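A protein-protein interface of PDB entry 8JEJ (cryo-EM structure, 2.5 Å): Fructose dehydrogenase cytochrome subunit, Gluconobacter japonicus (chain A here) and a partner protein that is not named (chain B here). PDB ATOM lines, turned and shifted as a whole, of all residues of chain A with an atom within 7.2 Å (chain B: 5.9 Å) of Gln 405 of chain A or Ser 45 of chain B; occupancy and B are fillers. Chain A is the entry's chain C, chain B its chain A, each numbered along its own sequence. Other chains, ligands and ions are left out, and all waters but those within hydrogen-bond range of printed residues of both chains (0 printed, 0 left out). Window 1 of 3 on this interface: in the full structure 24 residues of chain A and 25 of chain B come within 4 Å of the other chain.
The side-chain amide nitrogen (NE2) of Gln 405 of chain A sits at hydrogen-bond distance from the side-chain carboxylate (OD1) of Asp 43 of chain B, 3.4 Å away. O of Ala 341 of chain A lies within hydrogen-bond range of OG of Ser 45 of chain B (3.5 Å). The guanidinium group (NE) of Arg 44 of chain B is in hydrogen-bond range of the backbone carbonyl oxygen (O) of Val 404 of chain A. The backbone NH (N) of Leu 329 of chain A lies within hydrogen-bond range of the side-chain carboxylate (OD2) of Asp 43 of chain B (3.1 Å). The side-chain hydroxyl (OG1) of Thr 328 of chain A lies close to the side-chain carboxylate (OD2) of Asp 43 of chain B, 3.3 Å away. The backbone NH of Arg 44 of chain B lies within hydrogen-bond range of the side-chain amide oxygen of Gln 405 of chain A (3.1 Å). The side-chain amide oxygen (OE1) of Gln 405 of chain A lies within hydrogen-bond range of the backbone NH (N) of Ser 45 of chain B (3.1 Å).
The side-chain hydroxyl (OG) of Ser 402 of chain A is in hydrogen-bond range of the backbone NH (N) of Gln 405 of chain A. OD1 of Asn 50 of chain B is in hydrogen-bond range of NE2 of Gln 46 of chain B (2.7 Å). O of Leu 329 of chain A lies close to NE2 of Gln 411 of chain A (3.5 Å). The side-chain carboxylate (OE1) of Glu 49 of chain B sits at hydrogen-bond distance from the side-chain amide nitrogen (NE2) of Gln 46 of chain B. The side-chain hydroxyl of Ser 402 of chain A is in hydrogen-bond range of the backbone NH of Val 404 of chain A (3.3 Å).
Thr 328 of chain A touches Arg 42 of chain B. Leu 329 of chain A touches Ser 45 of chain B. CB of Leu 329 of chain A touches OE1 of Gln 46 of chain B (3.1 Å). Ser 45 of chain B touches Val 342 of chain A (OG to CG2, 3.4 Å).
Of the printed residues of chain A, Ser 45 of chain B touches Leu 329, Ala 341, Val 342 and Gln 405. Printed residues of chain B within 4 Å of Leu 329 of chain A: Asp 43, Ser 45 and Gln 46. Printed residues of chain A within 4 Å of Arg 42 of chain B: Thr 328 (3.98 Å). Of the printed residues of chain B, Val 342 of chain A touches Ser 45. Of the printed residues of chain B, Thr 328 of chain A touches Arg 42 (3.98 Å) and Asp 43 (3.2 Å). Of the printed residues of chain A, Asp 43 of chain B touches Thr 328 (3.2 Å), Leu 329 (3.1 Å) and Gln 405 (3.4 Å). Pro 400 of chain A touches none of the printed residues of chain B. Asp 401 of chain A touches none of the printed residues of chain B. The nearest residue of chain B that does not touch Gln 405 of chain A is Gln 46 of chain B (4.8 Å). The nearest printed residue of chain A that does not touch Asp 43 of chain B is Pro 406 of chain A (5.1 Å).
Of the 23 printed residues of chain A, 6 touch a printed residue of chain B. Hydrophobic or aromatic side chains of chain A within 4 Å of the printed part of chain B: Leu 329, Ala 341, Val 342 and Val 404. Among the printed residues, 11 pairs touch across the chains. Among the printed residues, no Asp or Glu carboxylate lies within 4 Å of a Lys or Arg side-chain nitrogen of the other chain.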
ATOM      1  N   THR A 328     -11.625   0.360   1.682  1.00  0.00           N
ATOM      2  CA  THR A 328     -12.159   1.188   2.772  1.00  0.00           C
ATOM      3  C   THR A 328     -11.282   2.430   2.999  1.00  0.00           C
ATOM      4  O   THR A 328     -10.580   2.591   3.996  1.00  0.00           O
ATOM      5  CB  THR A 328     -12.434   0.344   4.039  1.00  0.00           C
ATOM      6  OG1 THR A 328     -13.463   0.969   4.819  1.00  0.00           O
ATOM      7  CG2 THR A 328     -11.216   0.050   4.932  1.00  0.00           C
ATOM      8  N   LEU A 329     -11.352   3.321   2.003  1.00  0.00           N
ATOM      9  CA  LEU A 329     -10.492   4.501   1.939  1.00  0.00           C
ATOM     10  C   LEU A 329     -10.394   5.241   3.267  1.00  0.00           C
ATOM     11  O   LEU A 329     -11.383   5.762   3.789  1.00  0.00           O
ATOM     12  CB  LEU A 329     -10.966   5.464   0.838  1.00  0.00           C
ATOM     13  CG  LEU A 329     -12.376   6.060   0.701  1.00  0.00           C
ATOM     14  CD1 LEU A 329     -12.566   7.323   1.517  1.00  0.00           C
ATOM     15  CD2 LEU A 329     -12.640   6.370  -0.758  1.00  0.00           C
ATOM     16  N   ALA A 337      -8.936  13.914  -4.728  1.00  0.00           N
ATOM     17  CA  ALA A 337      -9.134  12.473  -4.856  1.00  0.00           C
ATOM     18  C   ALA A 337     -10.462  12.041  -4.248  1.00  0.00           C
ATOM     19  O   ALA A 337     -11.180  11.216  -4.826  1.00  0.00           O
ATOM     20  CB  ALA A 337      -7.974  11.725  -4.202  1.00  0.00           C
ATOM     21  N   LEU A 338     -10.803  12.585  -3.077  1.00  0.00           N
ATOM     22  CA  LEU A 338     -12.078  12.256  -2.450  1.00  0.00           C
ATOM     23  C   LEU A 338     -13.251  12.717  -3.304  1.00  0.00           C
ATOM     24  O   LEU A 338     -14.237  11.988  -3.464  1.00  0.00           O
ATOM     25  CB  LEU A 338     -12.150  12.878  -1.057  1.00  0.00           C
ATOM     26  CG  LEU A 338     -11.393  12.164   0.061  1.00  0.00           C
ATOM     27  CD1 LEU A 338     -11.272  13.069   1.272  1.00  0.00           C
ATOM     28  CD2 LEU A 338     -12.087  10.865   0.428  1.00  0.00           C
ATOM     29  N   GLU A 340     -13.243  13.110  -6.562  1.00  0.00           N
ATOM     30  CA  GLU A 340     -13.314  12.242  -7.731  1.00  0.00           C
ATOM     31  C   GLU A 340     -13.937  10.899  -7.382  1.00  0.00           C
ATOM     32  O   GLU A 340     -14.721  10.347  -8.162  1.00  0.00           O
ATOM     33  CB  GLU A 340     -11.925  12.049  -8.334  1.00  0.00           C
ATOM     34  CG  GLU A 340     -11.945  11.444  -9.727  1.00  0.00           C
ATOM     35  CD  GLU A 340     -12.129  12.483 -10.813  1.00  0.00           C
ATOM     36  OE1 GLU A 340     -12.156  13.688 -10.489  1.00  0.00           O
ATOM     37  OE2 GLU A 340     -12.245  12.096 -11.993  1.00  0.00           O
ATOM     38  N   ALA A 341     -13.603  10.357  -6.210  1.00  0.00           N
ATOM     39  CA  ALA A 341     -14.098   9.036  -5.844  1.00  0.00           C
ATOM     40  C   ALA A 341     -15.582   9.064  -5.499  1.00  0.00           C
ATOM     41  O   ALA A 341     -16.322   8.138  -5.851  1.00  0.00           O
ATOM     42  CB  ALA A 341     -13.285   8.479  -4.678  1.00  0.00           C
ATOM     43  N   VAL A 342     -16.041  10.114  -4.819  1.00  0.00           N
ATOM     44  CA  VAL A 342     -17.387  10.115  -4.255  1.00  0.00           C
ATOM     45  C   VAL A 342     -18.355  10.920  -5.115  1.00  0.00           C
ATOM     46  O   VAL A 342     -19.555  10.627  -5.153  1.00  0.00           O
ATOM     47  CB  VAL A 342     -17.368  10.649  -2.809  1.00  0.00           C
ATOM     48  CG1 VAL A 342     -18.718  10.446  -2.141  1.00  0.00           C
ATOM     49  CG2 VAL A 342     -16.276   9.962  -2.006  1.00  0.00           C
ATOM     50  N   CYS A 343     -17.851  11.930  -5.819  1.00  0.00           N
ATOM     51  CA  CYS A 343     -18.723  12.904  -6.462  1.00  0.00           C
ATOM     52  C   CYS A 343     -18.574  13.010  -7.969  1.00  0.00           C
ATOM     53  O   CYS A 343     -19.544  13.377  -8.635  1.00  0.00           O
ATOM     54  CB  CYS A 343     -18.495  14.299  -5.859  1.00  0.00           C
ATOM     55  SG  CYS A 343     -18.203  14.328  -4.069  1.00  0.00           S
ATOM     56  N   ILE A 380     -24.267  17.714   1.247  1.00  0.00           N
ATOM     57  CA  ILE A 380     -23.430  16.518   1.286  1.00  0.00           C
ATOM     58  C   ILE A 380     -23.945  15.544   2.341  1.00  0.00           C
ATOM     59  O   ILE A 380     -23.996  14.330   2.114  1.00  0.00           O
ATOM     60  CB  ILE A 380     -21.958  16.897   1.525  1.00  0.00           C
ATOM     61  CG1 ILE A 380     -21.425  17.710   0.345  1.00  0.00           C
ATOM     62  CG2 ILE A 380     -21.111  15.652   1.728  1.00  0.00           C
ATOM     63  CD1 ILE A 380     -20.074  18.329   0.596  1.00  0.00           C
ATOM     64  N   PRO A 396     -28.119  11.052  -3.250  1.00  0.00           N
ATOM     65  CA  PRO A 396     -28.025  10.258  -2.022  1.00  0.00           C
ATOM     66  C   PRO A 396     -27.310  11.005  -0.906  1.00  0.00           C
ATOM     67  O   PRO A 396     -26.487  11.893  -1.139  1.00  0.00           O
ATOM     68  CB  PRO A 396     -27.228   9.024  -2.459  1.00  0.00           C
ATOM     69  CG  PRO A 396     -26.445   9.484  -3.638  1.00  0.00           C
ATOM     70  CD  PRO A 396     -27.302  10.491  -4.339  1.00  0.00           C
ATOM     71  N   ALA A 397     -27.652  10.638   0.326  1.00  0.00           N
ATOM     72  CA  ALA A 397     -26.968  11.180   1.488  1.00  0.00           C
ATOM     73  C   ALA A 397     -25.568  10.592   1.606  1.00  0.00           C
ATOM     74  O   ALA A 397     -25.303   9.467   1.174  1.00  0.00           O
ATOM     75  CB  ALA A 397     -27.764  10.894   2.760  1.00  0.00           C
ATOM     76  N   PHE A 398     -24.660  11.372   2.195  1.00  0.00           N
ATOM     77  CA  PHE A 398     -23.286  10.929   2.401  1.00  0.00           C
ATOM     78  C   PHE A 398     -22.833  11.127   3.842  1.00  0.00           C
ATOM     79  O   PHE A 398     -21.630  11.195   4.103  1.00  0.00           O
ATOM     80  CB  PHE A 398     -22.336  11.646   1.439  1.00  0.00           C
ATOM     81  CG  PHE A 398     -22.524  11.249   0.006  1.00  0.00           C
ATOM     82  CD1 PHE A 398     -22.100  10.011  -0.443  1.00  0.00           C
ATOM     83  CD2 PHE A 398     -23.136  12.107  -0.891  1.00  0.00           C
ATOM     84  CE1 PHE A 398     -22.277   9.639  -1.758  1.00  0.00           C
ATOM     85  CE2 PHE A 398     -23.315  11.739  -2.207  1.00  0.00           C
ATOM     86  CZ  PHE A 398     -22.886  10.504  -2.639  1.00  0.00           C
ATOM     87  N   GLY A 399     -23.770  11.213   4.780  1.00  0.00           N
ATOM     88  CA  GLY A 399     -23.441  11.333   6.178  1.00  0.00           C
ATOM     89  C   GLY A 399     -23.165   9.984   6.809  1.00  0.00           C
ATOM     90  O   GLY A 399     -22.985   8.977   6.119  1.00  0.00           O
ATOM     91  N   PRO A 400     -23.115   9.943   8.142  1.00  0.00           N
ATOM     92  CA  PRO A 400     -22.866   8.663   8.825  1.00  0.00           C
ATOM     93  C   PRO A 400     -23.901   7.594   8.521  1.00  0.00           C
ATOM     94  O   PRO A 400     -23.557   6.406   8.488  1.00  0.00           O
ATOM     95  CB  PRO A 400     -22.882   9.052  10.311  1.00  0.00           C
ATOM     96  CG  PRO A 400     -22.590  10.510  10.330  1.00  0.00           C
ATOM     97  CD  PRO A 400     -23.194  11.072   9.083  1.00  0.00           C
ATOM     98  N   ASP A 401     -25.157   7.972   8.297  1.00  0.00           N
ATOM     99  CA  ASP A 401     -26.231   7.022   8.043  1.00  0.00           C
ATOM    100  C   ASP A 401     -26.352   6.644   6.572  1.00  0.00           C
ATOM    101  O   ASP A 401     -27.309   5.957   6.199  1.00  0.00           O
ATOM    102  CB  ASP A 401     -27.562   7.587   8.543  1.00  0.00           C
ATOM    103  CG  ASP A 401     -27.520   7.970  10.009  1.00  0.00           C
ATOM    104  OD1 ASP A 401     -26.581   7.542  10.711  1.00  0.00           O
ATOM    105  OD2 ASP A 401     -28.428   8.699  10.459  1.00  0.00           O
ATOM    106  N   SER A 402     -25.408   7.072   5.738  1.00  0.00           N
ATOM    107  CA  SER A 402     -25.499   6.853   4.301  1.00  0.00           C
ATOM    108  C   SER A 402     -25.470   5.367   3.961  1.00  0.00           C
ATOM    109  O   SER A 402     -24.855   4.555   4.656  1.00  0.00           O
ATOM    110  CB  SER A 402     -24.350   7.566   3.589  1.00  0.00           C
ATOM    111  OG  SER A 402     -24.441   7.409   2.185  1.00  0.00           O
ATOM    112  N   LEU A 403     -26.158   5.017   2.874  1.00  0.00           N
ATOM    113  CA  LEU A 403     -26.100   3.672   2.318  1.00  0.00           C
ATOM    114  C   LEU A 403     -25.072   3.545   1.207  1.00  0.00           C
ATOM    115  O   LEU A 403     -24.506   2.464   1.015  1.00  0.00           O
ATOM    116  CB  LEU A 403     -27.471   3.262   1.771  1.00  0.00           C
ATOM    117  CG  LEU A 403     -28.507   2.669   2.723  1.00  0.00           C
ATOM    118  CD1 LEU A 403     -29.616   2.016   1.922  1.00  0.00           C
ATOM    119  CD2 LEU A 403     -27.871   1.671   3.670  1.00  0.00           C
ATOM    120  N   VAL A 404     -24.819   4.626   0.473  1.00  0.00           N
ATOM    121  CA  VAL A 404     -23.924   4.566  -0.679  1.00  0.00           C
ATOM    122  C   VAL A 404     -22.471   4.683  -0.240  1.00  0.00           C
ATOM    123  O   VAL A 404     -21.647   3.807  -0.521  1.00  0.00           O
ATOM    124  CB  VAL A 404     -24.296   5.656  -1.701  1.00  0.00           C
ATOM    125  CG1 VAL A 404     -23.279   5.702  -2.826  1.00  0.00           C
ATOM    126  CG2 VAL A 404     -25.694   5.413  -2.244  1.00  0.00           C
ATOM    127  N   GLN A 405     -22.136   5.765   0.460  1.00  0.00           N
ATOM    128  CA  GLN A 405     -20.762   6.005   0.898  1.00  0.00           C
ATOM    129  C   GLN A 405     -20.783   6.904   2.121  1.00  0.00           C
ATOM    130  O   GLN A 405     -20.823   8.136   2.006  1.00  0.00           O
ATOM    131  CB  GLN A 405     -19.915   6.624  -0.211  1.00  0.00           C
ATOM    132  CG  GLN A 405     -18.466   6.856   0.178  1.00  0.00           C
ATOM    133  CD  GLN A 405     -17.822   5.624   0.778  1.00  0.00           C
ATOM    134  OE1 GLN A 405     -17.495   4.677   0.069  1.00  0.00           O
ATOM    135  NE2 GLN A 405     -17.633   5.634   2.091  1.00  0.00           N
ATOM    136  N   PRO A 406     -20.765   6.322   3.319  1.00  0.00           N
ATOM    137  CA  PRO A 406     -20.690   7.141   4.536  1.00  0.00           C
ATOM    138  C   PRO A 406     -19.352   7.862   4.622  1.00  0.00           C
ATOM    139  O   PRO A 406     -18.295   7.268   4.403  1.00  0.00           O
ATOM    140  CB  PRO A 406     -20.855   6.122   5.670  1.00  0.00           C
ATOM    141  CG  PRO A 406     -21.401   4.892   5.027  1.00  0.00           C
ATOM    142  CD  PRO A 406     -20.902   4.888   3.621  1.00  0.00           C
ATOM    143  N   LEU A 407     -19.405   9.146   4.956  1.00  0.00           N
ATOM    144  CA  LEU A 407     -18.217   9.974   5.078  1.00  0.00           C
ATOM    145  C   LEU A 407     -18.133  10.545   6.485  1.00  0.00           C
ATOM    146  O   LEU A 407     -19.155  10.856   7.102  1.00  0.00           O
ATOM    147  CB  LEU A 407     -18.220  11.115   4.057  1.00  0.00           C
ATOM    148  CG  LEU A 407     -18.369  10.759   2.578  1.00  0.00           C
ATOM    149  CD1 LEU A 407     -18.459  12.025   1.752  1.00  0.00           C
ATOM    150  CD2 LEU A 407     -17.214   9.894   2.111  1.00  0.00           C
ATOM    151  N   THR A 408     -16.910  10.671   6.988  1.00  0.00           N
ATOM    152  CA  THR A 408     -16.681  11.285   8.284  1.00  0.00           C
ATOM    153  C   THR A 408     -16.710  12.805   8.157  1.00  0.00           C
ATOM    154  O   THR A 408     -16.729  13.364   7.058  1.00  0.00           O
ATOM    155  CB  THR A 408     -15.350  10.820   8.871  1.00  0.00           C
ATOM    156  OG1 THR A 408     -14.270  11.396   8.127  1.00  0.00           O
ATOM    157  CG2 THR A 408     -15.243   9.307   8.809  1.00  0.00           C
ATOM    158  N   GLN A 411     -13.694  13.918   6.169  1.00  0.00           N
ATOM    159  CA  GLN A 411     -13.822  13.696   4.730  1.00  0.00           C
ATOM    160  C   GLN A 411     -14.800  14.682   4.102  1.00  0.00           C
ATOM    161  O   GLN A 411     -14.548  15.206   3.009  1.00  0.00           O
ATOM    162  CB  GLN A 411     -14.261  12.259   4.458  1.00  0.00           C
ATOM    163  CG  GLN A 411     -13.139  11.244   4.521  1.00  0.00           C
ATOM    164  CD  GLN A 411     -13.643   9.840   4.771  1.00  0.00           C
ATOM    165  OE1 GLN A 411     -14.783   9.642   5.186  1.00  0.00           O
ATOM    166  NE2 GLN A 411     -12.792   8.853   4.518  1.00  0.00           N
ATOM    167  N   ARG B  42     -15.461  -2.570   3.490  1.00  0.00           N
ATOM    168  CA  ARG B  42     -15.084  -1.993   2.209  1.00  0.00           C
ATOM    169  C   ARG B  42     -15.886  -0.727   1.946  1.00  0.00           C
ATOM    170  O   ARG B  42     -17.044  -0.610   2.353  1.00  0.00           O
ATOM    171  CB  ARG B  42     -15.295  -2.993   1.063  1.00  0.00           C
ATOM    172  CG  ARG B  42     -14.722  -4.373   1.336  1.00  0.00           C
ATOM    173  CD  ARG B  42     -14.490  -5.142   0.052  1.00  0.00           C
ATOM    174  NE  ARG B  42     -13.766  -6.385   0.283  1.00  0.00           N
ATOM    175  CZ  ARG B  42     -12.468  -6.546   0.069  1.00  0.00           C
ATOM    176  NH1 ARG B  42     -11.714  -5.553  -0.372  1.00  0.00           N
ATOM    177  NH2 ARG B  42     -11.913  -7.731   0.299  1.00  0.00           N
ATOM    178  N   ASP B  43     -15.251   0.221   1.264  1.00  0.00           N
ATOM    179  CA  ASP B  43     -15.881   1.470   0.857  1.00  0.00           C
ATOM    180  C   ASP B  43     -16.117   1.437  -0.645  1.00  0.00           C
ATOM    181  O   ASP B  43     -15.218   1.070  -1.407  1.00  0.00           O
ATOM    182  CB  ASP B  43     -15.013   2.675   1.227  1.00  0.00           C
ATOM    183  CG  ASP B  43     -15.167   3.085   2.678  1.00  0.00           C
ATOM    184  OD1 ASP B  43     -16.227   2.795   3.272  1.00  0.00           O
ATOM    185  OD2 ASP B  43     -14.229   3.699   3.225  1.00  0.00           O
ATOM    186  N   ARG B  44     -17.323   1.823  -1.064  1.00  0.00           N
ATOM    187  CA  ARG B  44     -17.664   1.790  -2.482  1.00  0.00           C
ATOM    188  C   ARG B  44     -16.770   2.720  -3.292  1.00  0.00           C
ATOM    189  O   ARG B  44     -16.283   2.345  -4.364  1.00  0.00           O
ATOM    190  CB  ARG B  44     -19.134   2.159  -2.673  1.00  0.00           C
ATOM    191  CG  ARG B  44     -19.459   2.766  -4.027  1.00  0.00           C
ATOM    192  CD  ARG B  44     -20.896   3.244  -4.082  1.00  0.00           C
ATOM    193  NE  ARG B  44     -21.759   2.462  -3.209  1.00  0.00           N
ATOM    194  CZ  ARG B  44     -22.421   1.376  -3.583  1.00  0.00           C
ATOM    195  NH1 ARG B  44     -22.360   0.923  -4.823  1.00  0.00           N
ATOM    196  NH2 ARG B  44     -23.160   0.727  -2.688  1.00  0.00           N
ATOM    197  N   SER B  45     -16.536   3.935  -2.793  1.00  0.00           N
ATOM    198  CA  SER B  45     -15.768   4.921  -3.550  1.00  0.00           C
ATOM    199  C   SER B  45     -14.321   4.482  -3.737  1.00  0.00           C
ATOM    200  O   SER B  45     -13.715   4.750  -4.782  1.00  0.00           O
ATOM    201  CB  SER B  45     -15.836   6.277  -2.853  1.00  0.00           C
ATOM    202  OG  SER B  45     -17.170   6.742  -2.795  1.00  0.00           O
ATOM    203  N   GLN B  46     -13.748   3.809  -2.738  1.00  0.00           N
ATOM    204  CA  GLN B  46     -12.397   3.283  -2.895  1.00  0.00           C
ATOM    205  C   GLN B  46     -12.348   2.191  -3.956  1.00  0.00           C
ATOM    206  O   GLN B  46     -11.397   2.127  -4.740  1.00  0.00           O
ATOM    207  CB  GLN B  46     -11.872   2.767  -1.557  1.00  0.00           C
ATOM    208  CG  GLN B  46     -10.408   2.363  -1.575  1.00  0.00           C
ATOM    209  CD  GLN B  46      -9.492   3.431  -2.148  1.00  0.00           C
ATOM    210  OE1 GLN B  46      -9.650   4.618  -1.872  1.00  0.00           O
ATOM    211  NE2 GLN B  46      -8.523   3.008  -2.948  1.00  0.00           N
ATOM    212  N   ILE B  47     -13.362   1.325  -4.001  1.00  0.00           N
ATOM    213  CA  ILE B  47     -13.425   0.318  -5.057  1.00  0.00           C
ATOM    214  C   ILE B  47     -13.564   0.987  -6.418  1.00  0.00           C
ATOM    215  O   ILE B  47     -12.997   0.526  -7.416  1.00  0.00           O
ATOM    216  CB  ILE B  47     -14.575  -0.674  -4.797  1.00  0.00           C
ATOM    217  CG1 ILE B  47     -14.496  -1.251  -3.380  1.00  0.00           C
ATOM    218  CG2 ILE B  47     -14.553  -1.787  -5.826  1.00  0.00           C
ATOM    219  CD1 ILE B  47     -13.137  -1.798  -3.000  1.00  0.00           C
ATOM    220  N   VAL B  48     -14.319   2.085  -6.478  1.00  0.00           N
ATOM    221  CA  VAL B  48     -14.478   2.821  -7.730  1.00  0.00           C
ATOM    222  C   VAL B  48     -13.136   3.370  -8.196  1.00  0.00           C
ATOM    223  O   VAL B  48     -12.768   3.258  -9.372  1.00  0.00           O
ATOM    224  CB  VAL B  48     -15.518   3.943  -7.559  1.00  0.00           C
ATOM    225  CG1 VAL B  48     -15.562   4.821  -8.791  1.00  0.00           C
ATOM    226  CG2 VAL B  48     -16.881   3.356  -7.277  1.00  0.00           C
ATOM    227  N   GLU B  49     -12.382   3.969  -7.271  1.00  0.00           N
ATOM    228  CA  GLU B  49     -11.057   4.479  -7.612  1.00  0.00           C
ATOM    229  C   GLU B  49     -10.124   3.353  -8.043  1.00  0.00           C
ATOM    230  O   GLU B  49      -9.354   3.506  -8.998  1.00  0.00           O
ATOM    231  CB  GLU B  49     -10.463   5.236  -6.427  1.00  0.00           C
ATOM    232  CG  GLU B  49      -9.137   5.907  -6.739  1.00  0.00           C
ATOM    233  CD  GLU B  49      -8.426   6.396  -5.498  1.00  0.00           C
ATOM    234  OE1 GLU B  49      -7.897   5.552  -4.745  1.00  0.00           O
ATOM    235  OE2 GLU B  49      -8.397   7.623  -5.274  1.00  0.00           O
ATOM    236  N   ASN B  50     -10.180   2.214  -7.349  1.00  0.00           N
ATOM    237  CA  ASN B  50      -9.335   1.080  -7.702  1.00  0.00           C
ATOM    238  C   ASN B  50      -9.658   0.561  -9.096  1.00  0.00           C
ATOM    239  O   ASN B  50      -8.755   0.179  -9.849  1.00  0.00           O
ATOM    240  CB  ASN B  50      -9.495  -0.037  -6.672  1.00  0.00           C
ATOM    241  CG  ASN B  50      -8.878   0.308  -5.337  1.00  0.00           C
ATOM    242  OD1 ASN B  50      -8.338   1.397  -5.153  1.00  0.00           O
ATOM    243  ND2 ASN B  50      -8.956  -0.620  -4.393  1.00  0.00           N
ATOM    244  N   PRO B 227     -20.728   3.285  -9.010  1.00  0.00           N
ATOM    245  CA  PRO B 227     -20.138   4.416  -8.282  1.00  0.00           C
ATOM    246  C   PRO B 227     -21.127   5.172  -7.419  1.00  0.00           C
ATOM    247  O   PRO B 227     -20.699   5.927  -6.539  1.00  0.00           O
ATOM    248  CB  PRO B 227     -19.588   5.316  -9.400  1.00  0.00           C
ATOM    249  CG  PRO B 227     -19.912   4.630 -10.697  1.00  0.00           C
ATOM    250  CD  PRO B 227     -20.943   3.594 -10.430  1.00  0.00           C
